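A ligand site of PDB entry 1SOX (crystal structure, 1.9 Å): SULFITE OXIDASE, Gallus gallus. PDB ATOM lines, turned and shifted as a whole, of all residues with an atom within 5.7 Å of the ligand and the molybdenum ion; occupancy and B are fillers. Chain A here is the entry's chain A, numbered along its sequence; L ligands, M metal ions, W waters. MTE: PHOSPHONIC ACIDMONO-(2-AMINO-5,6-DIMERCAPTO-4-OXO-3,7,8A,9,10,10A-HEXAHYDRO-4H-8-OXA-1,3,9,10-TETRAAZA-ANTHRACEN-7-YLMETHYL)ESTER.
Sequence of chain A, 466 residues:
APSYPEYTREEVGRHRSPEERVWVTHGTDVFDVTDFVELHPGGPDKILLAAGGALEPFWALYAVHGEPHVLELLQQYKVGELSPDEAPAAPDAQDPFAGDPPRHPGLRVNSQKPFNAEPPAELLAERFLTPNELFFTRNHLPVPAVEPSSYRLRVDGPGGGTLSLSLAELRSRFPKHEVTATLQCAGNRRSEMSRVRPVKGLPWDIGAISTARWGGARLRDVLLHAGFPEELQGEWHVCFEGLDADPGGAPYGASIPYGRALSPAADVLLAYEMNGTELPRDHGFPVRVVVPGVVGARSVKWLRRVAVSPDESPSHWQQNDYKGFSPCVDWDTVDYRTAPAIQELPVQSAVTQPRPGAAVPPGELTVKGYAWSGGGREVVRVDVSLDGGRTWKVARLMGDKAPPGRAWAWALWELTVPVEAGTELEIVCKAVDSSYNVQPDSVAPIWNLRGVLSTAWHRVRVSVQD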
ATOM      1  N   PHE A 135      34.611  23.572 -11.657  1.00  0.00           N
ATOM      2  CA  PHE A 135      33.231  23.782 -12.120  1.00  0.00           C
ATOM      3  C   PHE A 135      33.003  22.851 -13.306  1.00  0.00           C
ATOM      4  O   PHE A 135      33.871  22.806 -14.183  1.00  0.00           O
ATOM      5  CB  PHE A 135      33.029  25.251 -12.493  1.00  0.00           C
ATOM      6  CG  PHE A 135      31.606  25.705 -12.575  1.00  0.00           C
ATOM      7  CD1 PHE A 135      30.787  25.343 -13.627  1.00  0.00           C
ATOM      8  CD2 PHE A 135      31.085  26.537 -11.575  1.00  0.00           C
ATOM      9  CE1 PHE A 135      29.477  25.772 -13.707  1.00  0.00           C
ATOM     10  CE2 PHE A 135      29.775  26.974 -11.667  1.00  0.00           C
ATOM     11  CZ  PHE A 135      28.954  26.581 -12.715  1.00  0.00           C
ATOM     12  N   PHE A 136      31.891  22.104 -13.327  1.00  0.00           N
ATOM     13  CA  PHE A 136      31.709  21.178 -14.440  1.00  0.00           C
ATOM     14  C   PHE A 136      31.703  21.948 -15.758  1.00  0.00           C
ATOM     15  O   PHE A 136      31.264  23.102 -15.855  1.00  0.00           O
ATOM     16  CB  PHE A 136      30.444  20.363 -14.302  1.00  0.00           C
ATOM     17  CG  PHE A 136      29.191  20.959 -14.871  1.00  0.00           C
ATOM     18  CD1 PHE A 136      28.501  21.951 -14.176  1.00  0.00           C
ATOM     19  CD2 PHE A 136      28.680  20.523 -16.074  1.00  0.00           C
ATOM     20  CE1 PHE A 136      27.334  22.487 -14.673  1.00  0.00           C
ATOM     21  CE2 PHE A 136      27.509  21.054 -16.592  1.00  0.00           C
ATOM     22  CZ  PHE A 136      26.828  22.041 -15.884  1.00  0.00           C
ATOM     23  N   THR A 137      32.175  21.235 -16.787  1.00  0.00           N
ATOM     24  CA  THR A 137      32.271  21.838 -18.118  1.00  0.00           C
ATOM     25  C   THR A 137      31.524  21.015 -19.149  1.00  0.00           C
ATOM     26  O   THR A 137      31.688  19.786 -19.257  1.00  0.00           O
ATOM     27  CB  THR A 137      33.738  21.961 -18.544  1.00  0.00           C
ATOM     28  OG1 THR A 137      34.443  22.736 -17.548  1.00  0.00           O
ATOM     29  CG2 THR A 137      33.885  22.691 -19.880  1.00  0.00           C
ATOM     30  N   ARG A 138      30.711  21.690 -19.941  1.00  0.00           N
ATOM     31  CA  ARG A 138      29.916  21.043 -20.978  1.00  0.00           C
ATOM     32  C   ARG A 138      30.070  21.858 -22.262  1.00  0.00           C
ATOM     33  O   ARG A 138      29.529  22.949 -22.345  1.00  0.00           O
ATOM     34  CB  ARG A 138      28.456  20.940 -20.563  1.00  0.00           C
ATOM     35  CG  ARG A 138      27.637  19.844 -21.252  1.00  0.00           C
ATOM     36  CD  ARG A 138      27.341  20.196 -22.699  1.00  0.00           C
ATOM     37  NE  ARG A 138      26.500  19.245 -23.424  1.00  0.00           N
ATOM     38  CZ  ARG A 138      26.917  18.490 -24.440  1.00  0.00           C
ATOM     39  NH1 ARG A 138      28.185  18.542 -24.834  1.00  0.00           N
ATOM     40  NH2 ARG A 138      26.098  17.673 -25.095  1.00  0.00           N
ATOM     41  N   ASN A 139      30.868  21.313 -23.200  1.00  0.00           N
ATOM     42  CA  ASN A 139      31.078  22.005 -24.484  1.00  0.00           C
ATOM     43  C   ASN A 139      30.529  21.156 -25.618  1.00  0.00           C
ATOM     44  O   ASN A 139      30.854  19.955 -25.668  1.00  0.00           O
ATOM     45  CB  ASN A 139      32.572  22.209 -24.748  1.00  0.00           C
ATOM     46  CG  ASN A 139      33.265  23.139 -23.798  1.00  0.00           C
ATOM     47  OD1 ASN A 139      32.604  23.843 -23.013  1.00  0.00           O
ATOM     48  ND2 ASN A 139      34.593  23.177 -23.862  1.00  0.00           N
ATOM     49  N   HIS A 140      29.726  21.728 -26.517  1.00  0.00           N
ATOM     50  CA  HIS A 140      29.255  20.931 -27.638  1.00  0.00           C
ATOM     51  C   HIS A 140      30.282  20.975 -28.779  1.00  0.00           C
ATOM     52  O   HIS A 140      30.253  20.138 -29.678  1.00  0.00           O
ATOM     53  CB  HIS A 140      27.923  21.409 -28.179  1.00  0.00           C
ATOM     54  CG  HIS A 140      26.748  21.142 -27.294  1.00  0.00           C
ATOM     55  ND1 HIS A 140      26.411  21.956 -26.235  1.00  0.00           N
ATOM     56  CD2 HIS A 140      25.845  20.132 -27.307  1.00  0.00           C
ATOM     57  CE1 HIS A 140      25.351  21.443 -25.619  1.00  0.00           C
ATOM     58  NE2 HIS A 140      24.986  20.350 -26.255  1.00  0.00           N
ATOM     59  N   LEU A 141      31.108  22.007 -28.830  1.00  0.00           N
ATOM     60  CA  LEU A 141      32.038  22.314 -29.907  1.00  0.00           C
ATOM     61  C   LEU A 141      33.363  22.801 -29.400  1.00  0.00           C
ATOM     62  O   LEU A 141      33.584  22.947 -28.199  1.00  0.00           O
ATOM     63  CB  LEU A 141      31.364  23.465 -30.678  1.00  0.00           C
ATOM     64  CG  LEU A 141      30.005  23.172 -31.325  1.00  0.00           C
ATOM     65  CD1 LEU A 141      29.207  24.440 -31.530  1.00  0.00           C
ATOM     66  CD2 LEU A 141      30.193  22.374 -32.602  1.00  0.00           C
ATOM     67  N   LEU A 183      24.330  26.033 -11.843  1.00  0.00           N
ATOM     68  CA  LEU A 183      24.044  25.597 -13.208  1.00  0.00           C
ATOM     69  C   LEU A 183      23.985  24.064 -13.215  1.00  0.00           C
ATOM     70  O   LEU A 183      24.941  23.480 -12.713  1.00  0.00           O
ATOM     71  CB  LEU A 183      25.172  26.016 -14.168  1.00  0.00           C
ATOM     72  CG  LEU A 183      25.222  27.524 -14.483  1.00  0.00           C
ATOM     73  CD1 LEU A 183      26.273  27.817 -15.559  1.00  0.00           C
ATOM     74  CD2 LEU A 183      23.859  28.036 -14.922  1.00  0.00           C
ATOM     75  N   GLN A 184      22.881  23.504 -13.666  1.00  0.00           N
ATOM     76  CA  GLN A 184      22.755  22.060 -13.723  1.00  0.00           C
ATOM     77  C   GLN A 184      22.470  21.641 -15.163  1.00  0.00           C
ATOM     78  O   GLN A 184      21.531  22.135 -15.773  1.00  0.00           O
ATOM     79  CB  GLN A 184      21.596  21.546 -12.841  1.00  0.00           C
ATOM     80  CG  GLN A 184      21.570  20.010 -12.797  1.00  0.00           C
ATOM     81  CD  GLN A 184      20.416  19.419 -12.038  1.00  0.00           C
ATOM     82  OE1 GLN A 184      19.519  20.091 -11.497  1.00  0.00           O
ATOM     83  NE2 GLN A 184      20.429  18.081 -11.992  1.00  0.00           N
ATOM     84  N   CYS A 185      23.273  20.737 -15.706  1.00  0.00           N
ATOM     85  CA  CYS A 185      23.002  20.252 -17.071  1.00  0.00           C
ATOM     86  C   CYS A 185      21.780  19.372 -17.100  1.00  0.00           C
ATOM     87  O   CYS A 185      21.518  18.599 -16.162  1.00  0.00           O
ATOM     88  CB  CYS A 185      24.255  19.492 -17.530  1.00  0.00           C
ATOM     89  SG  CYS A 185      24.134  18.856 -19.200  1.00  0.00           S
ATOM     90  N   ALA A 186      20.986  19.365 -18.186  1.00  0.00           N
ATOM     91  CA  ALA A 186      19.831  18.496 -18.294  1.00  0.00           C
ATOM     92  C   ALA A 186      20.227  17.022 -18.173  1.00  0.00           C
ATOM     93  O   ALA A 186      19.407  16.180 -17.804  1.00  0.00           O
ATOM     94  CB  ALA A 186      19.122  18.663 -19.653  1.00  0.00           C
ATOM     95  N   GLY A 187      21.481  16.687 -18.495  1.00  0.00           N
ATOM     96  CA  GLY A 187      21.872  15.282 -18.395  1.00  0.00           C
ATOM     97  C   GLY A 187      22.473  14.883 -17.072  1.00  0.00           C
ATOM     98  O   GLY A 187      22.921  13.731 -16.972  1.00  0.00           O
ATOM     99  N   TRP A 214      28.176  34.865 -10.115  1.00  0.00           N
ATOM    100  CA  TRP A 214      28.374  35.474 -11.431  1.00  0.00           C
ATOM    101  C   TRP A 214      28.300  36.995 -11.384  1.00  0.00           C
ATOM    102  O   TRP A 214      27.447  37.517 -10.653  1.00  0.00           O
ATOM    103  CB  TRP A 214      27.320  34.947 -12.405  1.00  0.00           C
ATOM    104  CG  TRP A 214      27.245  33.448 -12.432  1.00  0.00           C
ATOM    105  CD1 TRP A 214      26.370  32.660 -11.730  1.00  0.00           C
ATOM    106  CD2 TRP A 214      28.113  32.556 -13.147  1.00  0.00           C
ATOM    107  NE1 TRP A 214      26.627  31.329 -11.987  1.00  0.00           N
ATOM    108  CE2 TRP A 214      27.698  31.247 -12.870  1.00  0.00           C
ATOM    109  CE3 TRP A 214      29.182  32.754 -14.039  1.00  0.00           C
ATOM    110  CZ2 TRP A 214      28.310  30.135 -13.443  1.00  0.00           C
ATOM    111  CZ3 TRP A 214      29.800  31.656 -14.602  1.00  0.00           C
ATOM    112  CH2 TRP A 214      29.379  30.341 -14.294  1.00  0.00           C
ATOM    113  N   GLY A 242      26.064  31.746 -29.725  1.00  0.00           N
ATOM    114  CA  GLY A 242      27.424  31.728 -29.273  1.00  0.00           C
ATOM    115  C   GLY A 242      28.373  31.844 -30.486  1.00  0.00           C
ATOM    116  O   GLY A 242      27.895  31.766 -31.616  1.00  0.00           O
ATOM    117  N   LEU A 243      29.633  32.034 -30.182  1.00  0.00           N
ATOM    118  CA  LEU A 243      30.678  32.141 -31.192  1.00  0.00           C
ATOM    119  C   LEU A 243      31.151  30.766 -31.659  1.00  0.00           C
ATOM    120  O   LEU A 243      31.895  30.672 -32.633  1.00  0.00           O
ATOM    121  CB  LEU A 243      31.910  32.887 -30.641  1.00  0.00           C
ATOM    122  CG  LEU A 243      31.715  34.396 -30.404  1.00  0.00           C
ATOM    123  CD1 LEU A 243      32.735  34.918 -29.417  1.00  0.00           C
ATOM    124  CD2 LEU A 243      31.767  35.148 -31.725  1.00  0.00           C
ATOM    125  N   ASP A 244      30.760  29.702 -30.973  1.00  0.00           N
ATOM    126  CA  ASP A 244      31.125  28.340 -31.354  1.00  0.00           C
ATOM    127  C   ASP A 244      30.107  27.824 -32.362  1.00  0.00           C
ATOM    128  O   ASP A 244      28.899  27.927 -32.152  1.00  0.00           O
ATOM    129  CB  ASP A 244      31.213  27.399 -30.147  1.00  0.00           C
ATOM    130  CG  ASP A 244      29.991  27.407 -29.251  1.00  0.00           C
ATOM    131  OD1 ASP A 244      29.285  28.430 -29.168  1.00  0.00           O
ATOM    132  OD2 ASP A 244      29.706  26.371 -28.604  1.00  0.00           O
ATOM    133  N   TYR A 252      26.019  27.536 -31.610  1.00  0.00           N
ATOM    134  CA  TYR A 252      25.184  27.026 -30.511  1.00  0.00           C
ATOM    135  C   TYR A 252      24.156  28.122 -30.208  1.00  0.00           C
ATOM    136  O   TYR A 252      24.540  29.292 -30.306  1.00  0.00           O
ATOM    137  CB  TYR A 252      26.055  26.707 -29.266  1.00  0.00           C
ATOM    138  CG  TYR A 252      25.165  26.172 -28.177  1.00  0.00           C
ATOM    139  CD1 TYR A 252      24.749  24.841 -28.167  1.00  0.00           C
ATOM    140  CD2 TYR A 252      24.682  27.014 -27.169  1.00  0.00           C
ATOM    141  CE1 TYR A 252      23.896  24.367 -27.182  1.00  0.00           C
ATOM    142  CE2 TYR A 252      23.846  26.523 -26.187  1.00  0.00           C
ATOM    143  CZ  TYR A 252      23.477  25.213 -26.179  1.00  0.00           C
ATOM    144  OH  TYR A 252      22.596  24.706 -25.217  1.00  0.00           O
ATOM    145  N   ASP A 282      36.720  28.080 -20.921  1.00  0.00           N
ATOM    146  CA  ASP A 282      35.802  26.930 -20.930  1.00  0.00           C
ATOM    147  C   ASP A 282      34.398  27.319 -20.476  1.00  0.00           C
ATOM    148  O   ASP A 282      33.413  26.672 -20.822  1.00  0.00           O
ATOM    149  CB  ASP A 282      36.334  25.812 -20.033  1.00  0.00           C
ATOM    150  CG  ASP A 282      37.085  24.710 -20.769  1.00  0.00           C
ATOM    151  OD1 ASP A 282      36.874  24.533 -21.975  1.00  0.00           O
ATOM    152  OD2 ASP A 282      37.902  24.018 -20.121  1.00  0.00           O
ATOM    153  N   HIS A 283      34.299  28.372 -19.651  1.00  0.00           N
ATOM    154  CA  HIS A 283      32.995  28.850 -19.185  1.00  0.00           C
ATOM    155  C   HIS A 283      32.488  30.082 -19.904  1.00  0.00           C
ATOM    156  O   HIS A 283      31.515  30.693 -19.425  1.00  0.00           O
ATOM    157  CB  HIS A 283      33.037  29.091 -17.667  1.00  0.00           C
ATOM    158  CG  HIS A 283      33.511  27.820 -16.992  1.00  0.00           C
ATOM    159  ND1 HIS A 283      32.720  26.702 -16.941  1.00  0.00           N
ATOM    160  CD2 HIS A 283      34.708  27.521 -16.448  1.00  0.00           C
ATOM    161  CE1 HIS A 283      33.420  25.743 -16.337  1.00  0.00           C
ATOM    162  NE2 HIS A 283      34.616  26.216 -16.006  1.00  0.00           N
ATOM    163  N   ARG A 288      28.997  35.403 -21.114  1.00  0.00           N
ATOM    164  CA  ARG A 288      28.043  34.341 -21.269  1.00  0.00           C
ATOM    165  C   ARG A 288      26.708  34.844 -20.689  1.00  0.00           C
ATOM    166  O   ARG A 288      26.716  35.761 -19.890  1.00  0.00           O
ATOM    167  CB  ARG A 288      28.404  33.030 -20.555  1.00  0.00           C
ATOM    168  CG  ARG A 288      28.244  33.128 -19.047  1.00  0.00           C
ATOM    169  CD  ARG A 288      28.486  31.830 -18.292  1.00  0.00           C
ATOM    170  NE  ARG A 288      27.630  30.746 -18.773  1.00  0.00           N
ATOM    171  CZ  ARG A 288      27.920  29.457 -18.549  1.00  0.00           C
ATOM    172  NH1 ARG A 288      29.018  29.123 -17.848  1.00  0.00           N
ATOM    173  NH2 ARG A 288      27.114  28.524 -19.017  1.00  0.00           N
ATOM    174  N   VAL A 295      17.676  25.287 -16.769  1.00  0.00           N
ATOM    175  CA  VAL A 295      18.621  24.266 -17.229  1.00  0.00           C
ATOM    176  C   VAL A 295      19.847  24.911 -17.852  1.00  0.00           C
ATOM    177  O   VAL A 295      19.747  25.928 -18.563  1.00  0.00           O
ATOM    178  CB  VAL A 295      17.934  23.258 -18.156  1.00  0.00           C
ATOM    179  CG1 VAL A 295      17.439  23.963 -19.433  1.00  0.00           C
ATOM    180  CG2 VAL A 295      18.898  22.118 -18.501  1.00  0.00           C
ATOM    181  N   GLY A 296      21.013  24.336 -17.600  1.00  0.00           N
ATOM    182  CA  GLY A 296      22.302  24.884 -18.048  1.00  0.00           C
ATOM    183  C   GLY A 296      22.326  25.154 -19.548  1.00  0.00           C
ATOM    184  O   GLY A 296      23.039  26.075 -19.966  1.00  0.00           O
ATOM    185  N   ALA A 297      21.615  24.374 -20.358  1.00  0.00           N
ATOM    186  CA  ALA A 297      21.656  24.542 -21.808  1.00  0.00           C
ATOM    187  C   ALA A 297      21.349  25.967 -22.275  1.00  0.00           C
ATOM    188  O   ALA A 297      21.799  26.359 -23.351  1.00  0.00           O
ATOM    189  CB  ALA A 297      20.657  23.602 -22.450  1.00  0.00           C
ATOM    190  N   ARG A 298      20.510  26.710 -21.551  1.00  0.00           N
ATOM    191  CA  ARG A 298      20.111  28.065 -21.948  1.00  0.00           C
ATOM    192  C   ARG A 298      21.103  29.144 -21.599  1.00  0.00           C
ATOM    193  O   ARG A 298      20.987  30.268 -22.120  1.00  0.00           O
ATOM    194  CB  ARG A 298      18.732  28.397 -21.387  1.00  0.00           C
ATOM    195  CG  ARG A 298      17.663  27.322 -21.527  1.00  0.00           C
ATOM    196  CD  ARG A 298      17.447  26.912 -23.003  1.00  0.00           C
ATOM    197  NE  ARG A 298      16.614  25.721 -23.057  1.00  0.00           N
ATOM    198  CZ  ARG A 298      16.604  24.733 -23.951  1.00  0.00           C
ATOM    199  NH1 ARG A 298      17.415  24.747 -24.986  1.00  0.00           N
ATOM    200  NH2 ARG A 298      15.763  23.708 -23.790  1.00  0.00           N
ATOM    201  N   SER A 299      22.130  28.860 -20.829  1.00  0.00           N
ATOM    202  CA  SER A 299      23.144  29.818 -20.426  1.00  0.00           C
ATOM    203  C   SER A 299      24.255  29.804 -21.485  1.00  0.00           C
ATOM    204  O   SER A 299      25.294  29.214 -21.263  1.00  0.00           O
ATOM    205  CB  SER A 299      23.708  29.531 -19.024  1.00  0.00           C
ATOM    206  OG  SER A 299      22.684  29.741 -18.033  1.00  0.00           O
ATOM    207  N   VAL A 300      23.972  30.456 -22.597  1.00  0.00           N
ATOM    208  CA  VAL A 300      24.908  30.456 -23.744  1.00  0.00           C
ATOM    209  C   VAL A 300      26.210  31.139 -23.489  1.00  0.00           C
ATOM    210  O   VAL A 300      26.261  32.271 -23.022  1.00  0.00           O
ATOM    211  CB  VAL A 300      24.159  31.064 -24.947  1.00  0.00           C
ATOM    212  CG1 VAL A 300      25.082  31.220 -26.141  1.00  0.00           C
ATOM    213  CG2 VAL A 300      22.923  30.219 -25.256  1.00  0.00           C
ATOM    214  N   LYS A 301      27.333  30.430 -23.750  1.00  0.00           N
ATOM    215  CA  LYS A 301      28.677  30.916 -23.530  1.00  0.00           C
ATOM    216  C   LYS A 301      29.237  31.557 -24.800  1.00  0.00           C
ATOM    217  O   LYS A 301      28.644  31.382 -25.863  1.00  0.00           O
ATOM    218  CB  LYS A 301      29.595  29.747 -23.131  1.00  0.00           C
ATOM    219  CG  LYS A 301      29.110  28.956 -21.914  1.00  0.00           C
ATOM    220  CD  LYS A 301      30.178  27.969 -21.462  1.00  0.00           C
ATOM    221  CE  LYS A 301      29.976  26.591 -22.090  1.00  0.00           C
ATOM    222  NZ  LYS A 301      30.917  25.579 -21.458  1.00  0.00           N
ATOM    223  N   TRP A 302      30.344  32.291 -24.686  1.00  0.00           N
ATOM    224  CA  TRP A 302      30.936  32.937 -25.866  1.00  0.00           C
ATOM    225  C   TRP A 302      29.864  33.690 -26.640  1.00  0.00           C
ATOM    226  O   TRP A 302      29.669  33.528 -27.843  1.00  0.00           O
ATOM    227  CB  TRP A 302      31.599  31.855 -26.763  1.00  0.00           C
ATOM    228  CG  TRP A 302      32.496  30.975 -25.943  1.00  0.00           C
ATOM    229  CD1 TRP A 302      33.652  31.322 -25.313  1.00  0.00           C
ATOM    230  CD2 TRP A 302      32.265  29.589 -25.639  1.00  0.00           C
ATOM    231  NE1 TRP A 302      34.147  30.236 -24.628  1.00  0.00           N
ATOM    232  CE2 TRP A 302      33.305  29.175 -24.806  1.00  0.00           C
ATOM    233  CE3 TRP A 302      31.282  28.678 -25.999  1.00  0.00           C
ATOM    234  CZ2 TRP A 302      33.427  27.867 -24.320  1.00  0.00           C
ATOM    235  CZ3 TRP A 302      31.364  27.386 -25.494  1.00  0.00           C
ATOM    236  CH2 TRP A 302      32.437  26.984 -24.686  1.00  0.00           C
ATOM    237  N   TYR A 322      16.909  18.482 -25.510  1.00  0.00           N
ATOM    238  CA  TYR A 322      16.543  19.015 -24.200  1.00  0.00           C
ATOM    239  C   TYR A 322      15.067  19.145 -23.958  1.00  0.00           C
ATOM    240  O   TYR A 322      14.547  20.195 -23.540  1.00  0.00           O
ATOM    241  CB  TYR A 322      17.280  20.344 -23.972  1.00  0.00           C
ATOM    242  CG  TYR A 322      18.781  20.207 -24.071  1.00  0.00           C
ATOM    243  CD1 TYR A 322      19.460  19.315 -23.263  1.00  0.00           C
ATOM    244  CD2 TYR A 322      19.529  20.922 -24.982  1.00  0.00           C
ATOM    245  CE1 TYR A 322      20.843  19.173 -23.350  1.00  0.00           C
ATOM    246  CE2 TYR A 322      20.896  20.807 -25.077  1.00  0.00           C
ATOM    247  CZ  TYR A 322      21.557  19.926 -24.243  1.00  0.00           C
ATOM    248  OH  TYR A 322      22.937  19.744 -24.315  1.00  0.00           O
HETATM  249  N1  MTE L   1      27.077  27.684 -24.823  1.00  0.00           N
HETATM  250  C2  MTE L   1      27.738  27.534 -26.029  1.00  0.00           C
HETATM  251  N2  MTE L   1      27.963  28.672 -26.726  1.00  0.00           N
HETATM  252  N3  MTE L   1      28.047  26.313 -26.476  1.00  0.00           N
HETATM  253  C4  MTE L   1      27.775  25.170 -25.749  1.00  0.00           C
HETATM  254  O4  MTE L   1      28.088  23.971 -26.145  1.00  0.00           O
HETATM  255  N5  MTE L   1      26.718  24.108 -23.545  1.00  0.00           N
HETATM  256  C6  MTE L   1      25.444  24.425 -22.663  1.00  0.00           C
HETATM  257  C7  MTE L   1      25.606  25.883 -21.901  1.00  0.00           C
HETATM  258  N8  MTE L   1      26.074  26.944 -22.744  1.00  0.00           N
HETATM  259  C9  MTE L   1      27.082  25.248 -24.446  1.00  0.00           C
HETATM  260  C10 MTE L   1      26.702  26.732 -23.961  1.00  0.00           C
HETATM  261  C1' MTE L   1      25.080  23.417 -21.780  1.00  0.00           C
HETATM  262  S1' MTE L   1      24.196  22.196 -22.446  1.00  0.00           S
HETATM  263  C2' MTE L   1      25.485  23.585 -20.379  1.00  0.00           C
HETATM  264  S2' MTE L   1      24.954  22.264 -19.348  1.00  0.00           S
HETATM  265  C3' MTE L   1      26.319  24.838 -19.865  1.00  0.00           C
HETATM  266  O3' MTE L   1      26.710  25.692 -20.969  1.00  0.00           O
HETATM  267  C4' MTE L   1      27.437  24.353 -19.158  1.00  0.00           C
HETATM  268  O4' MTE L   1      28.237  25.453 -18.684  1.00  0.00           O
HETATM  269  P   MTE L   1      29.496  25.305 -18.135  1.00  0.00           P
HETATM  270  O1P MTE L   1      29.349  24.421 -16.892  1.00  0.00           O
HETATM  271  O2P MTE L   1      30.127  26.589 -17.802  1.00  0.00           O
HETATM  272  O3P MTE L   1      30.314  24.666 -18.993  1.00  0.00           O
HETATM  273 MO    MO M   1      23.574  20.807 -20.607  1.00  0.00          MO
HETATM  274  O   HOH W   1      23.787  19.051 -21.992  1.00  0.00           O
HETATM  275  O   HOH W   2      31.340  24.427 -27.269  1.00  0.00           O
HETATM  276  O   HOH W   3      21.858  21.021 -20.448  1.00  0.00           O
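The backbone carbonyl oxygen of Phe 136 lies close to an oxygen (O1P) of the ligand, 2.5 Å away.
The backbone NH (N) of His 140 sits at hydrogen-bond distance from an oxygen (O4) of the ligand (2.8 Å).
An oxygen (O4) of the ligand lies within hydrogen-bond range of a ring nitrogen (ND1) of His 140, at 2.6 Å.
The backbone NH of Lys 301 sits at hydrogen-bond distance from a nitrogen (N1) of the ligand (3.0 Å).
The backbone carbonyl oxygen of Lys 301 is in hydrogen-bond range of a nitrogen (N2) of the ligand (2.9 Å).
The side-chain amino group (NZ) of Lys 301 is in salt-bridge range of an oxygen (O3P) of the ligand (2.7 Å).
OD2 of Asp 244 lies within hydrogen-bond range of N3 of the ligand (2.7 Å).
A ring nitrogen (ND1) of His 283 is in hydrogen-bond range of an oxygen (O2P) of the ligand (2.7 Å).
An oxygen (O2P) of the ligand is in salt-bridge range of the guanidinium group of Arg 288.
The backbone carbonyl oxygen (O) of Ser 299 lies within hydrogen-bond range of a nitrogen (N8) of the ligand.
N of Arg 138 sits at hydrogen-bond distance from O3P of the ligand, 3.1 Å away.
A nitrogen (N5) of the ligand sits at hydrogen-bond distance from the backbone carbonyl oxygen (O) of Arg 138.
S1' of the ligand sits close to OH of Tyr 322 (3.3 Å).
N of Gly 187 lies close to SG of Cys 185 (3.5 Å).
OH of Tyr 322 is in hydrogen-bond range of NE2 of His 140 (2.9 Å).
The backbone carbonyl oxygen (O) of Gln 184 lies within hydrogen-bond range of the backbone NH (N) of Gly 296 (2.9 Å).
The side-chain hydroxyl (OH) of Tyr 252 lies within hydrogen-bond range of the backbone carbonyl oxygen (O) of Ala 297 (2.6 Å).
The backbone NH (N) of Gly 242 lies within hydrogen-bond range of the backbone carbonyl oxygen (O) of Tyr 252 (2.9 Å).
O of Trp 302 is in hydrogen-bond range of N of Leu 243, 2.8 Å away.
OG1 of Thr 137 lies within hydrogen-bond range of O of Phe 135 (3.4 Å).
The side-chain amide nitrogen (ND2) of Asn 139 lies within hydrogen-bond range of the side-chain carboxylate (OD1) of Asp 282, 3.3 Å away.
Phe 135 touches the ligand (CE1 to O1P, 3.5 Å).
CA of Thr 137 touches O3P of the ligand (3.5 Å).
Asn 139 touches the ligand (C to O4, 3.8 Å).
Tyr 252 touches the ligand (CD2 to C2, 3.3 Å).
Gly 296 touches the ligand (O to C7, 3.2 Å).
CA of Ala 297 touches S1' of the ligand, at 3.5 Å.
CA of Val 300 touches N1 of the ligand, at 3.7 Å.
Trp 302 touches the ligand (CE3 to N2, 3.4 Å).
Within 4 Å of the ligand: Phe 135, Phe 136, Thr 137, Arg 138, Asn 139, His 140, Cys 185, Asp 244, Tyr 252, His 283, Arg 288, Gly 296, Ala 297, Ser 299, Val 300, Lys 301, Trp 302 and Tyr 322.
Residues that only touch the molybdenum ion: Ala 186 and Tyr 322.
Within 4 Å of the molybdenum ion: Cys 185, Ala 186 and Tyr 322.
The nearest printed residue that does not touch the molybdenum ion is Ala 297 (4.1 Å).
The molybdenum ion is bound by water W3 (1.7 Å), water W1 (2.2 Å), a sulfur (S2') of the ligand (2.4 Å), a sulfur (S1') of the ligand (2.4 Å) and the side-chain sulfur (SG) of Cys 185 (2.5 Å).
Water W3 lies within hydrogen-bond range of N of Ala 186 (2.9 Å) and N of Ala 297 (3.4 Å).
Water W1 bridges the side-chain hydroxyl of Tyr 322 (2.6 Å) and the guanidinium group of Arg 138 (3.1 Å).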
